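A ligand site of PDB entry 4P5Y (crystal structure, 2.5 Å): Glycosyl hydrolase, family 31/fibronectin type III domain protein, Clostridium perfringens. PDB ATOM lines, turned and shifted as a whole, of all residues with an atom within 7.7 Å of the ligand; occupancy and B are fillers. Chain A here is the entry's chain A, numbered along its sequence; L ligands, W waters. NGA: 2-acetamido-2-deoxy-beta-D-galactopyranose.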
ATOM      1  N   ALA A  35       2.816  19.533  -6.241  1.00  0.00           N
ATOM      2  CA  ALA A  35       2.266  20.859  -6.388  1.00  0.00           C
ATOM      3  C   ALA A  35       1.668  21.000  -7.782  1.00  0.00           C
ATOM      4  O   ALA A  35       2.098  20.300  -8.719  1.00  0.00           O
ATOM      5  CB  ALA A  35       3.332  21.916  -6.162  1.00  0.00           C
ATOM      6  N   ASP A  36       0.693  21.897  -7.902  1.00  0.00           N
ATOM      7  CA  ASP A  36       0.155  22.248  -9.204  1.00  0.00           C
ATOM      8  C   ASP A  36      -0.273  20.986  -9.948  1.00  0.00           C
ATOM      9  O   ASP A  36      -0.999  20.160  -9.404  1.00  0.00           O
ATOM     10  CB  ASP A  36       1.208  23.033  -9.990  1.00  0.00           C
ATOM     11  CG  ASP A  36       1.645  24.298  -9.257  1.00  0.00           C
ATOM     12  OD1 ASP A  36       0.739  24.975  -8.718  1.00  0.00           O
ATOM     13  OD2 ASP A  36       2.859  24.600  -9.208  1.00  0.00           O
ATOM     14  N   ASP A  38       2.132  18.963 -11.267  1.00  0.00           N
ATOM     15  CA  ASP A  38       3.399  18.265 -11.414  1.00  0.00           C
ATOM     16  C   ASP A  38       3.490  17.025 -10.520  1.00  0.00           C
ATOM     17  O   ASP A  38       4.171  17.015  -9.495  1.00  0.00           O
ATOM     18  CB  ASP A  38       4.524  19.246 -11.123  1.00  0.00           C
ATOM     19  CG  ASP A  38       4.534  20.400 -12.105  1.00  0.00           C
ATOM     20  OD1 ASP A  38       4.034  20.192 -13.227  1.00  0.00           O
ATOM     21  OD2 ASP A  38       5.015  21.503 -11.768  1.00  0.00           O
ATOM     22  N   ILE A  51       7.243  17.178 -15.282  1.00  0.00           N
ATOM     23  CA  ILE A  51       8.005  17.076 -14.047  1.00  0.00           C
ATOM     24  C   ILE A  51       7.141  16.682 -12.859  1.00  0.00           C
ATOM     25  O   ILE A  51       5.931  16.884 -12.841  1.00  0.00           O
ATOM     26  CB  ILE A  51       8.710  18.403 -13.694  1.00  0.00           C
ATOM     27  CG1 ILE A  51       7.682  19.443 -13.241  1.00  0.00           C
ATOM     28  CG2 ILE A  51       9.553  18.880 -14.881  1.00  0.00           C
ATOM     29  CD1 ILE A  51       8.263  20.813 -13.011  1.00  0.00           C
ATOM     30  N   HIS A  53       6.997  18.040  -9.105  1.00  0.00           N
ATOM     31  CA  HIS A  53       7.400  19.182  -8.300  1.00  0.00           C
ATOM     32  C   HIS A  53       6.738  19.000  -6.944  1.00  0.00           C
ATOM     33  O   HIS A  53       5.585  18.542  -6.879  1.00  0.00           O
ATOM     34  CB  HIS A  53       6.961  20.497  -8.964  1.00  0.00           C
ATOM     35  CG  HIS A  53       7.705  21.711  -8.483  1.00  0.00           C
ATOM     36  ND1 HIS A  53       7.633  22.163  -7.180  1.00  0.00           N
ATOM     37  CD2 HIS A  53       8.497  22.584  -9.143  1.00  0.00           C
ATOM     38  CE1 HIS A  53       8.368  23.251  -7.060  1.00  0.00           C
ATOM     39  NE2 HIS A  53       8.906  23.536  -8.239  1.00  0.00           N
ATOM     40  N   SER A  54       7.462  19.300  -5.865  1.00  0.00           N
ATOM     41  CA  SER A  54       6.902  19.168  -4.530  1.00  0.00           C
ATOM     42  C   SER A  54       6.237  20.480  -4.107  1.00  0.00           C
ATOM     43  O   SER A  54       6.397  21.512  -4.766  1.00  0.00           O
ATOM     44  CB  SER A  54       7.977  18.761  -3.519  1.00  0.00           C
ATOM     45  OG  SER A  54       8.986  19.754  -3.436  1.00  0.00           O
ATOM     46  N   ALA A  55       5.485  20.434  -3.011  1.00  0.00           N
ATOM     47  CA  ALA A  55       4.722  21.612  -2.593  1.00  0.00           C
ATOM     48  C   ALA A  55       5.657  22.751  -2.184  1.00  0.00           C
ATOM     49  O   ALA A  55       6.790  22.525  -1.744  1.00  0.00           O
ATOM     50  CB  ALA A  55       3.776  21.264  -1.451  1.00  0.00           C
ATOM     51  N   TYR A  56       5.180  23.984  -2.335  1.00  0.00           N
ATOM     52  CA  TYR A  56       5.968  25.143  -1.946  1.00  0.00           C
ATOM     53  C   TYR A  56       5.126  26.150  -1.188  1.00  0.00           C
ATOM     54  O   TYR A  56       5.288  27.351  -1.342  1.00  0.00           O
ATOM     55  CB  TYR A  56       6.621  25.798  -3.171  1.00  0.00           C
ATOM     56  CG  TYR A  56       5.683  26.017  -4.347  1.00  0.00           C
ATOM     57  CD1 TYR A  56       4.919  27.165  -4.462  1.00  0.00           C
ATOM     58  CD2 TYR A  56       5.573  25.064  -5.341  1.00  0.00           C
ATOM     59  CE1 TYR A  56       4.070  27.357  -5.535  1.00  0.00           C
ATOM     60  CE2 TYR A  56       4.724  25.242  -6.409  1.00  0.00           C
ATOM     61  CZ  TYR A  56       3.974  26.394  -6.513  1.00  0.00           C
ATOM     62  OH  TYR A  56       3.134  26.560  -7.597  1.00  0.00           O
ATOM     63  N   GLN A  57       4.217  25.636  -0.367  1.00  0.00           N
ATOM     64  CA  GLN A  57       3.488  26.503   0.558  1.00  0.00           C
ATOM     65  C   GLN A  57       4.428  26.969   1.673  1.00  0.00           C
ATOM     66  O   GLN A  57       5.615  26.606   1.688  1.00  0.00           O
ATOM     67  CB  GLN A  57       2.270  25.781   1.125  1.00  0.00           C
ATOM     68  CG  GLN A  57       1.327  25.226   0.052  1.00  0.00           C
ATOM     69  CD  GLN A  57       1.016  26.232  -1.056  1.00  0.00           C
ATOM     70  OE1 GLN A  57       0.865  27.427  -0.800  1.00  0.00           O
ATOM     71  NE2 GLN A  57       0.940  25.746  -2.297  1.00  0.00           N
ATOM     72  N   ARG A  84      14.552  19.563 -14.391  1.00  0.00           N
ATOM     73  CA  ARG A  84      13.543  20.371 -15.068  1.00  0.00           C
ATOM     74  C   ARG A  84      14.193  21.176 -16.186  1.00  0.00           C
ATOM     75  O   ARG A  84      15.126  21.929 -15.961  1.00  0.00           O
ATOM     76  CB  ARG A  84      12.879  21.292 -14.071  1.00  0.00           C
ATOM     77  CG  ARG A  84      11.672  22.038 -14.596  1.00  0.00           C
ATOM     78  CD  ARG A  84      11.282  23.101 -13.581  1.00  0.00           C
ATOM     79  NE  ARG A  84       9.926  23.585 -13.772  1.00  0.00           N
ATOM     80  CZ  ARG A  84       9.254  24.246 -12.833  1.00  0.00           C
ATOM     81  NH1 ARG A  84       9.813  24.495 -11.655  1.00  0.00           N
ATOM     82  NH2 ARG A  84       8.016  24.665 -13.074  1.00  0.00           N
ATOM     83  N   ASN A  86      12.820  23.603 -18.364  1.00  0.00           N
ATOM     84  CA  ASN A  86      12.450  24.990 -18.622  1.00  0.00           C
ATOM     85  C   ASN A  86      12.745  25.961 -17.479  1.00  0.00           C
ATOM     86  O   ASN A  86      12.509  27.160 -17.626  1.00  0.00           O
ATOM     87  CB  ASN A  86      10.957  25.101 -18.991  1.00  0.00           C
ATOM     88  CG  ASN A  86      10.026  24.403 -17.991  1.00  0.00           C
ATOM     89  OD1 ASN A  86      10.465  23.812 -16.996  1.00  0.00           O
ATOM     90  ND2 ASN A  86       8.736  24.482 -18.266  1.00  0.00           N
ATOM     91  N   SER A  87      13.266  25.457 -16.379  1.00  0.00           N
ATOM     92  CA  SER A  87      13.421  26.253 -15.166  1.00  0.00           C
ATOM     93  C   SER A  87      14.322  25.555 -14.165  1.00  0.00           C
ATOM     94  O   SER A  87      14.346  24.325 -14.101  1.00  0.00           O
ATOM     95  CB  SER A  87      12.055  26.513 -14.523  1.00  0.00           C
ATOM     96  OG  SER A  87      12.181  27.066 -13.216  1.00  0.00           O
ATOM     97  N   ARG A  88      15.055  26.336 -13.383  1.00  0.00           N
ATOM     98  CA  ARG A  88      15.932  25.774 -12.358  1.00  0.00           C
ATOM     99  C   ARG A  88      15.196  25.497 -11.040  1.00  0.00           C
ATOM    100  O   ARG A  88      15.763  24.930 -10.117  1.00  0.00           O
ATOM    101  CB  ARG A  88      17.123  26.691 -12.092  1.00  0.00           C
ATOM    102  CG  ARG A  88      16.755  28.129 -11.739  1.00  0.00           C
ATOM    103  CD  ARG A  88      16.422  28.292 -10.274  1.00  0.00           C
ATOM    104  NE  ARG A  88      15.939  29.645  -9.977  1.00  0.00           N
ATOM    105  CZ  ARG A  88      16.669  30.599  -9.405  1.00  0.00           C
ATOM    106  NH1 ARG A  88      17.908  30.360  -9.035  1.00  0.00           N
ATOM    107  NH2 ARG A  88      16.138  31.802  -9.198  1.00  0.00           N
ATOM    108  N   ASN A  89      13.937  25.902 -10.960  1.00  0.00           N
ATOM    109  CA  ASN A  89      13.174  25.706  -9.737  1.00  0.00           C
ATOM    110  C   ASN A  89      12.967  24.231  -9.384  1.00  0.00           C
ATOM    111  O   ASN A  89      12.262  23.500 -10.086  1.00  0.00           O
ATOM    112  CB  ASN A  89      11.829  26.427  -9.829  1.00  0.00           C
ATOM    113  CG  ASN A  89      11.920  27.874  -9.374  1.00  0.00           C
ATOM    114  OD1 ASN A  89      13.019  28.411  -9.238  1.00  0.00           O
ATOM    115  ND2 ASN A  89      10.771  28.499  -9.126  1.00  0.00           N
ATOM    116  N   GLY A  90      13.596  23.817  -8.296  1.00  0.00           N
ATOM    117  CA  GLY A  90      13.534  22.453  -7.830  1.00  0.00           C
ATOM    118  C   GLY A  90      14.737  21.645  -8.274  1.00  0.00           C
ATOM    119  O   GLY A  90      14.787  20.431  -8.033  1.00  0.00           O
ATOM    120  N   LEU A 149      17.907  23.937  -5.659  1.00  0.00           N
ATOM    121  CA  LEU A 149      17.865  25.313  -6.160  1.00  0.00           C
ATOM    122  C   LEU A 149      16.446  25.798  -6.442  1.00  0.00           C
ATOM    123  O   LEU A 149      15.554  25.002  -6.723  1.00  0.00           O
ATOM    124  CB  LEU A 149      18.662  25.457  -7.446  1.00  0.00           C
ATOM    125  CG  LEU A 149      20.130  25.067  -7.470  1.00  0.00           C
ATOM    126  CD1 LEU A 149      20.647  25.242  -8.878  1.00  0.00           C
ATOM    127  CD2 LEU A 149      20.896  25.918  -6.507  1.00  0.00           C
ATOM    128  N   GLY A 150      16.265  27.116  -6.413  1.00  0.00           N
ATOM    129  CA  GLY A 150      15.032  27.725  -6.881  1.00  0.00           C
ATOM    130  C   GLY A 150      15.023  29.188  -6.494  1.00  0.00           C
ATOM    131  O   GLY A 150      15.938  29.644  -5.814  1.00  0.00           O
ATOM    132  N   ASP A 151      13.998  29.915  -6.910  1.00  0.00           N
ATOM    133  CA  ASP A 151      13.828  31.297  -6.466  1.00  0.00           C
ATOM    134  C   ASP A 151      13.981  31.366  -4.954  1.00  0.00           C
ATOM    135  O   ASP A 151      14.459  32.359  -4.419  1.00  0.00           O
ATOM    136  CB  ASP A 151      12.470  31.845  -6.882  1.00  0.00           C
ATOM    137  CG  ASP A 151      12.265  31.762  -8.373  1.00  0.00           C
ATOM    138  OD1 ASP A 151      13.247  31.976  -9.123  1.00  0.00           O
ATOM    139  OD2 ASP A 151      11.134  31.468  -8.800  1.00  0.00           O
ATOM    140  N   THR A 152      13.565  30.303  -4.276  1.00  0.00           N
ATOM    141  CA  THR A 152      13.937  30.090  -2.889  1.00  0.00           C
ATOM    142  C   THR A 152      14.690  28.782  -2.868  1.00  0.00           C
ATOM    143  O   THR A 152      14.185  27.776  -3.337  1.00  0.00           O
ATOM    144  CB  THR A 152      12.716  30.018  -1.944  1.00  0.00           C
ATOM    145  OG1 THR A 152      11.814  31.086  -2.256  1.00  0.00           O
ATOM    146  CG2 THR A 152      13.159  30.119  -0.491  1.00  0.00           C
ATOM    147  N   LYS A 155      13.921  24.604  -0.581  1.00  0.00           N
ATOM    148  CA  LYS A 155      12.544  24.518  -0.114  1.00  0.00           C
ATOM    149  C   LYS A 155      11.761  23.454  -0.875  1.00  0.00           C
ATOM    150  O   LYS A 155      11.046  22.658  -0.288  1.00  0.00           O
ATOM    151  CB  LYS A 155      11.850  25.874  -0.231  1.00  0.00           C
ATOM    152  CG  LYS A 155      10.377  25.880   0.194  1.00  0.00           C
ATOM    153  CD  LYS A 155       9.817  27.300   0.077  1.00  0.00           C
ATOM    154  CE  LYS A 155       8.370  27.406   0.533  1.00  0.00           C
ATOM    155  NZ  LYS A 155       8.235  27.390   2.016  1.00  0.00           N
ATOM    156  N   TYR A 156      11.916  23.429  -2.194  1.00  0.00           N
ATOM    157  CA  TYR A 156      11.157  22.492  -2.998  1.00  0.00           C
ATOM    158  C   TYR A 156      12.029  21.772  -4.025  1.00  0.00           C
ATOM    159  O   TYR A 156      13.064  22.283  -4.439  1.00  0.00           O
ATOM    160  CB  TYR A 156       9.987  23.215  -3.692  1.00  0.00           C
ATOM    161  CG  TYR A 156      10.340  24.574  -4.235  1.00  0.00           C
ATOM    162  CD1 TYR A 156      11.044  24.707  -5.430  1.00  0.00           C
ATOM    163  CD2 TYR A 156       9.966  25.711  -3.564  1.00  0.00           C
ATOM    164  CE1 TYR A 156      11.365  25.963  -5.929  1.00  0.00           C
ATOM    165  CE2 TYR A 156      10.279  26.964  -4.052  1.00  0.00           C
ATOM    166  CZ  TYR A 156      10.975  27.093  -5.236  1.00  0.00           C
ATOM    167  OH  TYR A 156      11.279  28.346  -5.703  1.00  0.00           O
ATOM    168  N   ALA A 157      11.597  20.573  -4.419  1.00  0.00           N
ATOM    169  CA  ALA A 157      12.331  19.789  -5.405  1.00  0.00           C
ATOM    170  C   ALA A 157      11.462  19.448  -6.610  1.00  0.00           C
ATOM    171  O   ALA A 157      10.241  19.293  -6.520  1.00  0.00           O
ATOM    172  CB  ALA A 157      12.865  18.522  -4.790  1.00  0.00           C
ATOM    173  N   SER A 158      12.128  19.320  -7.760  1.00  0.00           N
ATOM    174  CA  SER A 158      11.494  18.764  -8.942  1.00  0.00           C
ATOM    175  C   SER A 158      12.428  17.767  -9.621  1.00  0.00           C
ATOM    176  O   SER A 158      13.633  17.732  -9.358  1.00  0.00           O
ATOM    177  CB  SER A 158      11.070  19.882  -9.909  1.00  0.00           C
ATOM    178  OG  SER A 158      12.153  20.733 -10.247  1.00  0.00           O
HETATM  179  C1  NGA L   1       6.556  28.815  -9.875  1.00  0.00           C
HETATM  180  C2  NGA L   1       6.712  27.500 -10.641  1.00  0.00           C
HETATM  181  C3  NGA L   1       6.414  26.331  -9.702  1.00  0.00           C
HETATM  182  C4  NGA L   1       7.264  26.455  -8.432  1.00  0.00           C
HETATM  183  C5  NGA L   1       7.007  27.813  -7.807  1.00  0.00           C
HETATM  184  C6  NGA L   1       7.767  28.013  -6.498  1.00  0.00           C
HETATM  185  C7  NGA L   1       6.348  27.680 -13.060  1.00  0.00           C
HETATM  186  C8  NGA L   1       5.326  27.695 -14.160  1.00  0.00           C
HETATM  187  N2  NGA L   1       5.869  27.449 -11.830  1.00  0.00           N
HETATM  188  O1  NGA L   1       6.962  29.902 -10.679  1.00  0.00           O
HETATM  189  O3  NGA L   1       6.637  25.096 -10.342  1.00  0.00           O
HETATM  190  O4  NGA L   1       8.630  26.348  -8.768  1.00  0.00           O
HETATM  191  O5  NGA L   1       7.390  28.803  -8.739  1.00  0.00           O
HETATM  192  O6  NGA L   1       8.389  29.287  -6.475  1.00  0.00           O
HETATM  193  O7  NGA L   1       7.541  27.882 -13.318  1.00  0.00           O
HETATM  194  O   HOH W   1       4.905  23.327  -9.676  1.00  0.00           O
HETATM  195  O   HOH W   2       9.598  30.323  -4.141  1.00  0.00           O
HETATM  196  O   HOH W   3       5.821  32.961 -10.140  1.00  0.00           O
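A ring nitrogen (NE2) of His 53 sits at hydrogen-bond distance from an oxygen (O4) of the ligand.
ND2 of Asn 89 is in hydrogen-bond range of O4 of the ligand.
An oxygen (O3) of the ligand lies within hydrogen-bond range of the guanidinium group (NH2) of Arg 84, 3.1 Å away.
OH of Tyr 156 is in hydrogen-bond range of O6 of the ligand, at 3.1 Å.
The backbone NH of His 53 sits at hydrogen-bond distance from the backbone carbonyl oxygen of Asp 38, 3.0 Å away.
The backbone NH of Ala 35 is in hydrogen-bond range of the backbone carbonyl oxygen of His 53.
O of Asn 89 is in hydrogen-bond range of NH1 of Arg 84, at 3.1 Å.
ND2 of Asn 89 is in hydrogen-bond range of OH of Tyr 156, 3.5 Å away.
The guanidinium group (NE) of Arg 88 lies within hydrogen-bond range of the side-chain amide oxygen (OD1) of Asn 89 (3.3 Å).
The side-chain amide oxygen (OD1) of Asn 86 lies close to the guanidinium group (NE) of Arg 84.
The backbone NH (N) of Asp 151 sits at hydrogen-bond distance from the side-chain hydroxyl (OH) of Tyr 156 (3.4 Å).
The side-chain hydroxyl of Tyr 156 lies within hydrogen-bond range of the backbone NH of Thr 152, at 3.3 Å.
Merely in contact with the ligand: Tyr 56 (3.5 Å) and Asp 36 (3.98 Å).
Hydrophobic or aromatic side chains within 4 Å of the ligand: His 53, Tyr 56 and Tyr 156.
Six residues have an atom within 4 Å of the ligand: Asp 36, His 53, Tyr 56, Arg 84, Asn 89 and Tyr 156.
Along chain A the residues within 4 Å of the ligand span positions 36 to 156.
Water W1 lies within hydrogen-bond range of the side-chain carboxylate of Asp 36 (2.5 Å), an oxygen (O3) of the ligand (2.6 Å) and the side-chain carboxylate of Asp 38 (2.8 Å).
Water W2 lies within hydrogen-bond range of O6 of the ligand, OG1 of Thr 152 and OH of Tyr 156.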
